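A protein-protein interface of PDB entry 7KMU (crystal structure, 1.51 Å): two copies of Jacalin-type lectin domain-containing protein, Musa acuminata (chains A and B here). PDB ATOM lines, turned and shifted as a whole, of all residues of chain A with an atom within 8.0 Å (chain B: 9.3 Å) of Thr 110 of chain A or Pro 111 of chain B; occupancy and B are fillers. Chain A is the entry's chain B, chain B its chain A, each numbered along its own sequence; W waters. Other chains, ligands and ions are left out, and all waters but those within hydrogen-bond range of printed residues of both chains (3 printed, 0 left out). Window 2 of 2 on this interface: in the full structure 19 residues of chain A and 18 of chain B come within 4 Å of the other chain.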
ATOM      1  N   TRP A  10      18.113  11.143  24.203  1.00  0.00           N
ATOM      2  CA  TRP A  10      18.585  10.888  22.850  1.00  0.00           C
ATOM      3  C   TRP A  10      19.160  12.221  22.395  1.00  0.00           C
ATOM      4  O   TRP A  10      18.561  13.268  22.664  1.00  0.00           O
ATOM      5  CB  TRP A  10      17.452  10.479  21.914  1.00  0.00           C
ATOM      6  CG  TRP A  10      16.832   9.177  22.309  1.00  0.00           C
ATOM      7  CD1 TRP A  10      17.244   7.925  21.947  1.00  0.00           C
ATOM      8  CD2 TRP A  10      15.734   8.994  23.209  1.00  0.00           C
ATOM      9  NE1 TRP A  10      16.444   6.975  22.536  1.00  0.00           N
ATOM     10  CE2 TRP A  10      15.498   7.603  23.304  1.00  0.00           C
ATOM     11  CE3 TRP A  10      14.898   9.877  23.918  1.00  0.00           C
ATOM     12  CZ2 TRP A  10      14.478   7.071  24.099  1.00  0.00           C
ATOM     13  CZ3 TRP A  10      13.903   9.349  24.726  1.00  0.00           C
ATOM     14  CH2 TRP A  10      13.722   7.958  24.841  1.00  0.00           C
ATOM     15  N   GLY A  11      20.331  12.192  21.769  1.00  0.00           N
ATOM     16  CA  GLY A  11      20.982  13.409  21.293  1.00  0.00           C
ATOM     17  C   GLY A  11      22.444  13.475  21.662  1.00  0.00           C
ATOM     18  O   GLY A  11      23.034  12.477  22.092  1.00  0.00           O
ATOM     19  N   GLY A  78      12.008  10.923  16.496  1.00  0.00           N
ATOM     20  CA  GLY A  78      12.839  11.909  15.831  1.00  0.00           C
ATOM     21  C   GLY A  78      14.157  11.363  15.362  1.00  0.00           C
ATOM     22  O   GLY A  78      14.338  10.144  15.281  1.00  0.00           O
ATOM     23  N   HIS A  79      15.093  12.287  15.055  1.00  0.00           N
ATOM     24  CA  HIS A  79      16.425  11.943  14.580  1.00  0.00           C
ATOM     25  C   HIS A  79      17.499  12.677  15.342  1.00  0.00           C
ATOM     26  O   HIS A  79      17.366  13.883  15.584  1.00  0.00           O
ATOM     27  CB  HIS A  79      16.579  12.290  13.087  1.00  0.00           C
ATOM     28  CG  HIS A  79      15.962  11.282  12.180  1.00  0.00           C
ATOM     29  ND1 HIS A  79      16.742  10.365  11.488  1.00  0.00           N
ATOM     30  CD2 HIS A  79      14.658  11.058  11.895  1.00  0.00           C
ATOM     31  CE1 HIS A  79      15.887   9.629  10.788  1.00  0.00           C
ATOM     32  NE2 HIS A  79      14.623  10.001  11.008  1.00  0.00           N
ATOM     33  N   VAL A  80      18.581  11.959  15.689  1.00  0.00           N
ATOM     34  CA  VAL A  80      19.810  12.538  16.254  1.00  0.00           C
ATOM     35  C   VAL A  80      20.679  12.754  15.018  1.00  0.00           C
ATOM     36  O   VAL A  80      20.879  11.815  14.237  1.00  0.00           O
ATOM     37  CB  VAL A  80      20.499  11.648  17.296  1.00  0.00           C
ATOM     38  CG1 VAL A  80      21.814  12.286  17.751  1.00  0.00           C
ATOM     39  CG2 VAL A  80      19.575  11.401  18.486  1.00  0.00           C
ATOM     40  N   VAL A  81      21.169  13.979  14.810  1.00  0.00           N
ATOM     41  CA  VAL A  81      21.876  14.322  13.583  1.00  0.00           C
ATOM     42  C   VAL A  81      23.167  15.056  13.793  1.00  0.00           C
ATOM     43  O   VAL A  81      23.408  15.629  14.865  1.00  0.00           O
ATOM     44  CB  VAL A  81      20.960  15.190  12.656  1.00  0.00           C
ATOM     45  CG1 VAL A  81      19.570  14.579  12.510  1.00  0.00           C
ATOM     46  CG2 VAL A  81      20.859  16.648  13.138  1.00  0.00           C
ATOM     47  N   ASP A  82      23.982  15.084  12.721  1.00  0.00           N
ATOM     48  CA  ASP A  82      25.214  15.861  12.700  1.00  0.00           C
ATOM     49  C   ASP A  82      24.852  17.176  12.006  1.00  0.00           C
ATOM     50  O   ASP A  82      24.357  17.158  10.873  1.00  0.00           O
ATOM     51  CB  ASP A  82      26.329  15.129  11.937  1.00  0.00           C
ATOM     52  CG  ASP A  82      27.649  15.871  11.986  1.00  0.00           C
ATOM     53  OD1 ASP A  82      27.832  16.811  11.183  1.00  0.00           O
ATOM     54  OD2 ASP A  82      28.491  15.524  12.839  1.00  0.00           O
ATOM     55  N   THR A  87      26.216  17.386  17.474  1.00  0.00           N
ATOM     56  CA  THR A  87      25.300  16.241  17.473  1.00  0.00           C
ATOM     57  C   THR A  87      24.060  16.735  18.226  1.00  0.00           C
ATOM     58  O   THR A  87      24.134  16.980  19.429  1.00  0.00           O
ATOM     59  CB  THR A  87      25.942  15.008  18.145  1.00  0.00           C
ATOM     60  OG1 THR A  87      27.137  14.652  17.440  1.00  0.00           O
ATOM     61  CG2 THR A  87      25.012  13.802  18.169  1.00  0.00           C
ATOM     62  N   ILE A  88      22.944  16.936  17.517  1.00  0.00           N
ATOM     63  CA  ILE A  88      21.732  17.533  18.104  1.00  0.00           C
ATOM     64  C   ILE A  88      20.467  16.819  17.586  1.00  0.00           C
ATOM     65  O   ILE A  88      20.559  15.880  16.793  1.00  0.00           O
ATOM     66  CB  ILE A  88      21.685  19.066  17.769  1.00  0.00           C
ATOM     67  CG1 ILE A  88      21.543  19.311  16.252  1.00  0.00           C
ATOM     68  CG2 ILE A  88      22.912  19.842  18.340  1.00  0.00           C
ATOM     69  CD1 ILE A  88      21.260  20.770  15.872  1.00  0.00           C
ATOM     70  N   ILE A  89      19.288  17.304  17.996  1.00  0.00           N
ATOM     71  CA  ILE A  89      18.013  16.767  17.491  1.00  0.00           C
ATOM     72  C   ILE A  89      17.690  17.512  16.182  1.00  0.00           C
ATOM     73  O   ILE A  89      17.568  18.747  16.167  1.00  0.00           O
ATOM     74  CB  ILE A  89      16.889  16.908  18.549  1.00  0.00           C
ATOM     75  CG1 ILE A  89      17.284  16.270  19.906  1.00  0.00           C
ATOM     76  CG2 ILE A  89      15.548  16.324  18.011  1.00  0.00           C
ATOM     77  CD1 ILE A  89      17.712  14.751  19.819  1.00  0.00           C
ATOM     78  N   GLY A  90      17.571  16.751  15.090  1.00  0.00           N
ATOM     79  CA  GLY A  90      17.324  17.323  13.773  1.00  0.00           C
ATOM     80  C   GLY A  90      15.885  17.243  13.311  1.00  0.00           C
ATOM     81  O   GLY A  90      15.476  18.030  12.451  1.00  0.00           O
ATOM     82  N   LYS A  91      15.111  16.274  13.861  1.00  0.00           N
ATOM     83  CA  LYS A  91      13.701  16.074  13.526  1.00  0.00           C
ATOM     84  C   LYS A  91      12.981  15.619  14.773  1.00  0.00           C
ATOM     85  O   LYS A  91      13.556  14.883  15.578  1.00  0.00           O
ATOM     86  CB  LYS A  91      13.530  15.002  12.442  1.00  0.00           C
ATOM     87  CG  LYS A  91      13.645  15.551  11.044  1.00  0.00           C
ATOM     88  CD  LYS A  91      13.149  14.548  10.006  1.00  0.00           C
ATOM     89  CE  LYS A  91      13.290  15.161   8.652  1.00  0.00           C
ATOM     90  NZ  LYS A  91      12.771  14.273   7.584  1.00  0.00           N
ATOM     91  N   TYR A 107      16.740  17.631   8.906  1.00  0.00           N
ATOM     92  CA  TYR A 107      17.880  16.721   8.946  1.00  0.00           C
ATOM     93  C   TYR A 107      17.550  15.350   9.507  1.00  0.00           C
ATOM     94  O   TYR A 107      16.784  15.235  10.464  1.00  0.00           O
ATOM     95  CB  TYR A 107      19.019  17.335   9.782  1.00  0.00           C
ATOM     96  CG  TYR A 107      19.981  18.222   9.019  1.00  0.00           C
ATOM     97  CD1 TYR A 107      19.525  19.326   8.300  1.00  0.00           C
ATOM     98  CD2 TYR A 107      21.355  18.028   9.111  1.00  0.00           C
ATOM     99  CE1 TYR A 107      20.410  20.178   7.642  1.00  0.00           C
ATOM    100  CE2 TYR A 107      22.251  18.868   8.450  1.00  0.00           C
ATOM    101  CZ  TYR A 107      21.773  19.941   7.716  1.00  0.00           C
ATOM    102  OH  TYR A 107      22.650  20.772   7.064  1.00  0.00           O
ATOM    103  N   GLU A 108      18.174  14.304   8.936  1.00  0.00           N
ATOM    104  CA  GLU A 108      18.030  12.941   9.429  1.00  0.00           C
ATOM    105  C   GLU A 108      19.401  12.383   9.834  1.00  0.00           C
ATOM    106  O   GLU A 108      20.446  12.959   9.490  1.00  0.00           O
ATOM    107  CB  GLU A 108      17.300  12.031   8.419  1.00  0.00           C
ATOM    108  CG  GLU A 108      15.825  12.386   8.282  1.00  0.00           C
ATOM    109  CD  GLU A 108      14.921  11.397   7.569  1.00  0.00           C
ATOM    110  OE1 GLU A 108      15.420  10.351   7.095  1.00  0.00           O
ATOM    111  OE2 GLU A 108      13.701  11.664   7.499  1.00  0.00           O
ATOM    112  N   GLY A 109      19.387  11.311  10.604  1.00  0.00           N
ATOM    113  CA  GLY A 109      20.606  10.682  11.092  1.00  0.00           C
ATOM    114  C   GLY A 109      20.288   9.361  11.741  1.00  0.00           C
ATOM    115  O   GLY A 109      19.954   8.395  11.040  1.00  0.00           O
ATOM    116  N   THR A 110      20.344   9.317  13.084  1.00  0.00           N
ATOM    117  CA  THR A 110      20.038   8.099  13.825  1.00  0.00           C
ATOM    118  C   THR A 110      18.635   8.245  14.409  1.00  0.00           C
ATOM    119  O   THR A 110      18.431   9.107  15.260  1.00  0.00           O
ATOM    120  CB  THR A 110      21.084   7.822  14.917  1.00  0.00           C
ATOM    121  OG1 THR A 110      22.380   7.792  14.309  1.00  0.00           O
ATOM    122  CG2 THR A 110      20.848   6.495  15.626  1.00  0.00           C
ATOM    123  N   PRO A 111      17.640   7.474  13.940  1.00  0.00           N
ATOM    124  CA  PRO A 111      16.292   7.632  14.490  1.00  0.00           C
ATOM    125  C   PRO A 111      16.144   7.106  15.903  1.00  0.00           C
ATOM    126  O   PRO A 111      16.880   6.220  16.336  1.00  0.00           O
ATOM    127  CB  PRO A 111      15.416   6.829  13.529  1.00  0.00           C
ATOM    128  CG  PRO A 111      16.323   5.770  13.013  1.00  0.00           C
ATOM    129  CD  PRO A 111      17.680   6.427  12.893  1.00  0.00           C
ATOM    130  N   PHE A 112      15.181   7.683  16.621  1.00  0.00           N
ATOM    131  CA  PHE A 112      14.764   7.235  17.943  1.00  0.00           C
ATOM    132  C   PHE A 112      13.242   7.282  17.972  1.00  0.00           C
ATOM    133  O   PHE A 112      12.615   8.100  17.270  1.00  0.00           O
ATOM    134  CB  PHE A 112      15.366   8.058  19.092  1.00  0.00           C
ATOM    135  CG  PHE A 112      15.042   9.536  19.113  1.00  0.00           C
ATOM    136  CD1 PHE A 112      15.829  10.443  18.419  1.00  0.00           C
ATOM    137  CD2 PHE A 112      13.968  10.022  19.861  1.00  0.00           C
ATOM    138  CE1 PHE A 112      15.534  11.812  18.443  1.00  0.00           C
ATOM    139  CE2 PHE A 112      13.664  11.388  19.876  1.00  0.00           C
ATOM    140  CZ  PHE A 112      14.454  12.275  19.167  1.00  0.00           C
ATOM    141  N   SER A 113      12.635   6.401  18.772  1.00  0.00           N
ATOM    142  CA  SER A 113      11.188   6.338  18.874  1.00  0.00           C
ATOM    143  C   SER A 113      10.780   5.786  20.214  1.00  0.00           C
ATOM    144  O   SER A 113      11.374   4.803  20.697  1.00  0.00           O
ATOM    145  CB  SER A 113      10.595   5.498  17.749  1.00  0.00           C
ATOM    146  OG  SER A 113      11.100   4.168  17.772  1.00  0.00           O
ATOM    147  N   TRP B  10       8.944  -2.402  19.214  1.00  0.00           N
ATOM    148  CA  TRP B  10       9.759  -2.114  18.041  1.00  0.00           C
ATOM    149  C   TRP B  10       9.856  -3.476  17.348  1.00  0.00           C
ATOM    150  O   TRP B  10      10.092  -4.486  18.024  1.00  0.00           O
ATOM    151  CB  TRP B  10      11.170  -1.611  18.399  1.00  0.00           C
ATOM    152  CG  TRP B  10      11.160  -0.306  19.132  1.00  0.00           C
ATOM    153  CD1 TRP B  10      11.145   0.953  18.591  1.00  0.00           C
ATOM    154  CD2 TRP B  10      11.172  -0.136  20.554  1.00  0.00           C
ATOM    155  NE1 TRP B  10      11.134   1.899  19.599  1.00  0.00           N
ATOM    156  CE2 TRP B  10      11.192   1.256  20.811  1.00  0.00           C
ATOM    157  CE3 TRP B  10      11.214  -1.028  21.641  1.00  0.00           C
ATOM    158  CZ2 TRP B  10      11.203   1.771  22.114  1.00  0.00           C
ATOM    159  CZ3 TRP B  10      11.245  -0.513  22.929  1.00  0.00           C
ATOM    160  CH2 TRP B  10      11.244   0.869  23.154  1.00  0.00           C
ATOM    161  N   GLY B  11       9.632  -3.509  16.033  1.00  0.00           N
ATOM    162  CA  GLY B  11       9.693  -4.750  15.272  1.00  0.00           C
ATOM    163  C   GLY B  11       8.488  -4.920  14.372  1.00  0.00           C
ATOM    164  O   GLY B  11       7.664  -4.006  14.241  1.00  0.00           O
ATOM    165  N   MET B  76      17.825  -0.786  26.796  1.00  0.00           N
ATOM    166  CA  MET B  76      17.736  -1.797  25.759  1.00  0.00           C
ATOM    167  C   MET B  76      17.937  -1.078  24.443  1.00  0.00           C
ATOM    168  O   MET B  76      17.395   0.010  24.257  1.00  0.00           O
ATOM    169  CB  MET B  76      16.388  -2.519  25.764  1.00  0.00           C
ATOM    170  CG  MET B  76      16.232  -3.510  24.602  1.00  0.00           C
ATOM    171  SD  MET B  76      14.652  -4.406  24.666  1.00  0.00           S
ATOM    172  CE  MET B  76      13.515  -3.113  24.184  1.00  0.00           C
ATOM    173  N   GLU B  77      18.731  -1.647  23.536  1.00  0.00           N
ATOM    174  CA  GLU B  77      18.904  -1.026  22.221  1.00  0.00           C
ATOM    175  C   GLU B  77      19.084  -2.107  21.167  1.00  0.00           C
ATOM    176  O   GLU B  77      19.569  -3.198  21.471  1.00  0.00           O
ATOM    177  CB  GLU B  77      20.061  -0.007  22.225  1.00  0.00           C
ATOM    178  CG  GLU B  77      21.424  -0.632  22.390  1.00  0.00           C
ATOM    179  CD  GLU B  77      22.515   0.385  22.637  1.00  0.00           C
ATOM    180  OE1 GLU B  77      23.036   0.948  21.648  1.00  0.00           O
ATOM    181  OE2 GLU B  77      22.845   0.623  23.821  1.00  0.00           O
ATOM    182  N   GLY B  78      18.709  -1.805  19.936  1.00  0.00           N
ATOM    183  CA  GLY B  78      18.880  -2.800  18.890  1.00  0.00           C
ATOM    184  C   GLY B  78      18.475  -2.287  17.541  1.00  0.00           C
ATOM    185  O   GLY B  78      18.377  -1.077  17.340  1.00  0.00           O
ATOM    186  N   HIS B  79      18.216  -3.213  16.623  1.00  0.00           N
ATOM    187  CA  HIS B  79      17.821  -2.880  15.262  1.00  0.00           C
ATOM    188  C   HIS B  79      16.635  -3.700  14.850  1.00  0.00           C
ATOM    189  O   HIS B  79      16.605  -4.917  15.098  1.00  0.00           O
ATOM    190  CB  HIS B  79      18.970  -3.187  14.273  1.00  0.00           C
ATOM    191  CG  HIS B  79      20.044  -2.151  14.237  1.00  0.00           C
ATOM    192  ND1 HIS B  79      20.152  -1.258  13.185  1.00  0.00           N
ATOM    193  CD2 HIS B  79      21.033  -1.901  15.128  1.00  0.00           C
ATOM    194  CE1 HIS B  79      21.199  -0.498  13.467  1.00  0.00           C
ATOM    195  NE2 HIS B  79      21.746  -0.833  14.637  1.00  0.00           N
ATOM    196  N   VAL B  80      15.684  -3.039  14.163  1.00  0.00           N
ATOM    197  CA  VAL B  80      14.556  -3.672  13.493  1.00  0.00           C
ATOM    198  C   VAL B  80      15.080  -3.875  12.070  1.00  0.00           C
ATOM    199  O   VAL B  80      15.560  -2.923  11.432  1.00  0.00           O
ATOM    200  CB  VAL B  80      13.287  -2.806  13.513  1.00  0.00           C
ATOM    201  CG1 VAL B  80      12.190  -3.428  12.642  1.00  0.00           C
ATOM    202  CG2 VAL B  80      12.793  -2.624  14.939  1.00  0.00           C
ATOM    203  N   VAL B  81      15.049  -5.122  11.596  1.00  0.00           N
ATOM    204  CA  VAL B  81      15.673  -5.459  10.315  1.00  0.00           C
ATOM    205  C   VAL B  81      14.770  -6.167   9.352  1.00  0.00           C
ATOM    206  O   VAL B  81      13.762  -6.747   9.745  1.00  0.00           O
ATOM    207  CB  VAL B  81      16.977  -6.290  10.529  1.00  0.00           C
ATOM    208  CG1 VAL B  81      17.867  -5.669  11.600  1.00  0.00           C
ATOM    209  CG2 VAL B  81      16.679  -7.760  10.860  1.00  0.00           C
ATOM    210  N   ILE B  89      13.661  -8.509  14.931  1.00  0.00           N
ATOM    211  CA  ILE B  89      14.771  -7.920  15.684  1.00  0.00           C
ATOM    212  C   ILE B  89      16.071  -8.587  15.217  1.00  0.00           C
ATOM    213  O   ILE B  89      16.222  -9.803  15.345  1.00  0.00           O
ATOM    214  CB  ILE B  89      14.543  -8.048  17.214  1.00  0.00           C
ATOM    215  CG1 ILE B  89      13.197  -7.436  17.655  1.00  0.00           C
ATOM    216  CG2 ILE B  89      15.729  -7.436  18.002  1.00  0.00           C
ATOM    217  CD1 ILE B  89      12.959  -5.942  17.186  1.00  0.00           C
ATOM    218  N   GLY B  90      16.994  -7.789  14.667  1.00  0.00           N
ATOM    219  CA  GLY B  90      18.250  -8.309  14.127  1.00  0.00           C
ATOM    220  C   GLY B  90      19.468  -8.166  15.017  1.00  0.00           C
ATOM    221  O   GLY B  90      20.457  -8.887  14.848  1.00  0.00           O
ATOM    222  N   LYS B  91      19.434  -7.188  15.942  1.00  0.00           N
ATOM    223  CA  LYS B  91      20.526  -6.922  16.871  1.00  0.00           C
ATOM    224  C   LYS B  91      19.888  -6.483  18.182  1.00  0.00           C
ATOM    225  O   LYS B  91      18.851  -5.818  18.156  1.00  0.00           O
ATOM    226  CB  LYS B  91      21.441  -5.802  16.330  1.00  0.00           C
ATOM    227  CG  LYS B  91      22.869  -5.804  16.855  1.00  0.00           C
ATOM    228  CD  LYS B  91      23.841  -4.990  15.942  1.00  0.00           C
ATOM    229  CE  LYS B  91      24.404  -5.730  14.736  1.00  0.00           C
ATOM    230  NZ  LYS B  91      25.633  -5.046  14.196  1.00  0.00           N
ATOM    231  N   TYR B 107      22.554  -8.427  11.876  1.00  0.00           N
ATOM    232  CA  TYR B 107      21.795  -7.617  10.933  1.00  0.00           C
ATOM    233  C   TYR B 107      21.494  -6.251  11.498  1.00  0.00           C
ATOM    234  O   TYR B 107      21.290  -6.114  12.709  1.00  0.00           O
ATOM    235  CB  TYR B 107      20.478  -8.309  10.545  1.00  0.00           C
ATOM    236  CG  TYR B 107      20.562  -9.196   9.314  1.00  0.00           C
ATOM    237  CD1 TYR B 107      21.476 -10.243   9.245  1.00  0.00           C
ATOM    238  CD2 TYR B 107      19.685  -9.023   8.249  1.00  0.00           C
ATOM    239  CE1 TYR B 107      21.552 -11.064   8.117  1.00  0.00           C
ATOM    240  CE2 TYR B 107      19.736  -9.851   7.127  1.00  0.00           C
ATOM    241  CZ  TYR B 107      20.676 -10.864   7.065  1.00  0.00           C
ATOM    242  OH  TYR B 107      20.735 -11.675   5.952  1.00  0.00           O
ATOM    243  N   GLU B 108      21.452  -5.240  10.627  1.00  0.00           N
ATOM    244  CA  GLU B 108      21.099  -3.882  11.012  1.00  0.00           C
ATOM    245  C   GLU B 108      19.951  -3.384  10.137  1.00  0.00           C
ATOM    246  O   GLU B 108      19.638  -3.988   9.104  1.00  0.00           O
ATOM    247  CB  GLU B 108      22.311  -2.930  10.949  1.00  0.00           C
ATOM    248  CG  GLU B 108      23.339  -3.246  12.020  1.00  0.00           C
ATOM    249  CD  GLU B 108      24.522  -2.301  12.105  1.00  0.00           C
ATOM    250  OE1 GLU B 108      24.581  -1.334  11.314  1.00  0.00           O
ATOM    251  OE2 GLU B 108      25.390  -2.525  12.975  1.00  0.00           O
ATOM    252  N   GLY B 109      19.302  -2.314  10.571  1.00  0.00           N
ATOM    253  CA  GLY B 109      18.185  -1.747   9.844  1.00  0.00           C
ATOM    254  C   GLY B 109      17.837  -0.391  10.392  1.00  0.00           C
ATOM    255  O   GLY B 109      18.554   0.588  10.146  1.00  0.00           O
ATOM    256  N   THR B 110      16.749  -0.344  11.159  1.00  0.00           N
ATOM    257  CA  THR B 110      16.277   0.872  11.820  1.00  0.00           C
ATOM    258  C   THR B 110      16.592   0.717  13.308  1.00  0.00           C
ATOM    259  O   THR B 110      15.995  -0.139  13.977  1.00  0.00           O
ATOM    260  CB  THR B 110      14.782   1.098  11.580  1.00  0.00           C
ATOM    261  OG1 THR B 110      14.531   1.098  10.166  1.00  0.00           O
ATOM    262  CG2 THR B 110      14.279   2.401  12.208  1.00  0.00           C
ATOM    263  N   PRO B 111      17.492   1.549  13.866  1.00  0.00           N
ATOM    264  CA  PRO B 111      17.807   1.405  15.285  1.00  0.00           C
ATOM    265  C   PRO B 111      16.693   1.875  16.208  1.00  0.00           C
ATOM    266  O   PRO B 111      15.881   2.750  15.867  1.00  0.00           O
ATOM    267  CB  PRO B 111      19.057   2.272  15.463  1.00  0.00           C
ATOM    268  CG  PRO B 111      18.977   3.285  14.377  1.00  0.00           C
ATOM    269  CD  PRO B 111      18.317   2.592  13.218  1.00  0.00           C
ATOM    270  N   PHE B 112      16.684   1.292  17.410  1.00  0.00           N
ATOM    271  CA  PHE B 112      15.825   1.720  18.511  1.00  0.00           C
ATOM    272  C   PHE B 112      16.661   1.669  19.788  1.00  0.00           C
ATOM    273  O   PHE B 112      17.628   0.909  19.889  1.00  0.00           O
ATOM    274  CB  PHE B 112      14.542   0.875  18.654  1.00  0.00           C
ATOM    275  CG  PHE B 112      14.781  -0.583  18.950  1.00  0.00           C
ATOM    276  CD1 PHE B 112      14.940  -1.497  17.922  1.00  0.00           C
ATOM    277  CD2 PHE B 112      14.839  -1.047  20.264  1.00  0.00           C
ATOM    278  CE1 PHE B 112      15.160  -2.852  18.198  1.00  0.00           C
ATOM    279  CE2 PHE B 112      15.065  -2.397  20.538  1.00  0.00           C
ATOM    280  CZ  PHE B 112      15.228  -3.295  19.503  1.00  0.00           C
ATOM    281  N   SER B 113      16.306   2.518  20.751  1.00  0.00           N
ATOM    282  CA  SER B 113      16.988   2.565  22.029  1.00  0.00           C
ATOM    283  C   SER B 113      16.070   3.128  23.078  1.00  0.00           C
ATOM    284  O   SER B 113      15.338   4.098  22.828  1.00  0.00           O
ATOM    285  CB  SER B 113      18.254   3.409  21.941  1.00  0.00           C
ATOM    286  OG  SER B 113      17.978   4.731  21.513  1.00  0.00           O
ATOM    287  N   ILE B 114      16.127   2.530  24.260  1.00  0.00           N
ATOM    288  CA  ILE B 114      15.313   2.981  25.374  1.00  0.00           C
ATOM    289  C   ILE B 114      16.185   3.086  26.645  1.00  0.00           C
ATOM    290  O   ILE B 114      16.125   2.235  27.540  1.00  0.00           O
ATOM    291  CB  ILE B 114      13.988   2.174  25.531  1.00  0.00           C
ATOM    292  CG1 ILE B 114      13.078   2.760  26.629  1.00  0.00           C
ATOM    293  CG2 ILE B 114      14.193   0.662  25.716  1.00  0.00           C
ATOM    294  CD1 ILE B 114      12.452   4.126  26.201  1.00  0.00           C
HETATM  295  O   HOH W   1      13.411   3.870  16.100  1.00  0.00           O
HETATM  296  O   HOH W   2      14.063   4.468  20.439  1.00  0.00           O
HETATM  297  O   HOH W   3      18.079   5.049  18.655  1.00  0.00           O
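Water W1 lies within hydrogen-bond range of the backbone carbonyl oxygen of Pro 111 of chain B and the side-chain hydroxyl of Ser 113 of chain A. Water W2 bridges O of Ser 113 of chain A (2.7 Å) and O of Ser 113 of chain B (2.7 Å). Water W3 lies within hydrogen-bond range of the backbone carbonyl oxygen (O) of Pro 111 of chain A (2.9 Å) and the side-chain hydroxyl (OG) of Ser 113 of chain B (2.9 Å).
The side-chain hydroxyl of Ser 113 of chain A sits at hydrogen-bond distance from the indole nitrogen of Trp 10 of chain B (2.9 Å). OG of Ser 113 of chain B lies within hydrogen-bond range of NE1 of Trp 10 of chain A, 2.9 Å away.
Of the printed residues of chain B, Thr 110 of chain A touches Pro 111. Of chain A, only Thr 110 and Pro 111 come within 4 Å of Pro 111 of chain B. Of the printed residues of chain A, Ser 113 of chain B touches Trp 10 (2.9 Å). Printed residues of chain B within 4 Å of Trp 10 of chain A: Ser 113 (2.9 Å).
N of Thr 110 of chain A sits at hydrogen-bond distance from O of Val 80 of chain A (2.8 Å).
Trp 10 of chain A touches Ser 113 of chain B, and with the chains exchanged Ser 113 of chain A touches Trp 10 of chain B. Thr 110 of chain A touches Pro 111 of chain B, but with the chains exchanged Pro 111 of chain A does not touch Thr 110 of chain B (4.02 Å). Pro 111 of chain A touches its own counterpart, Pro 111 of chain B. 16 positions are printed for both chains. Of the 4 pairs that touch across the chains among the printed residues, 3 have their exchanged pair printed and touching as well.
Of the 19 printed residues of chain B, 3 touch a printed residue of chain A. Hydrophobic or aromatic side chains of chain B within 4 Å of the printed part of chain A: Trp 10 and Pro 111. Hydrophobic or aromatic side chains of chain A that line the printed part of chain B: Trp 10 and Pro 111.
Pro 111 of chain B touches Thr 110 of chain A. Pro 111 of chain B touches Pro 111 of chain A.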
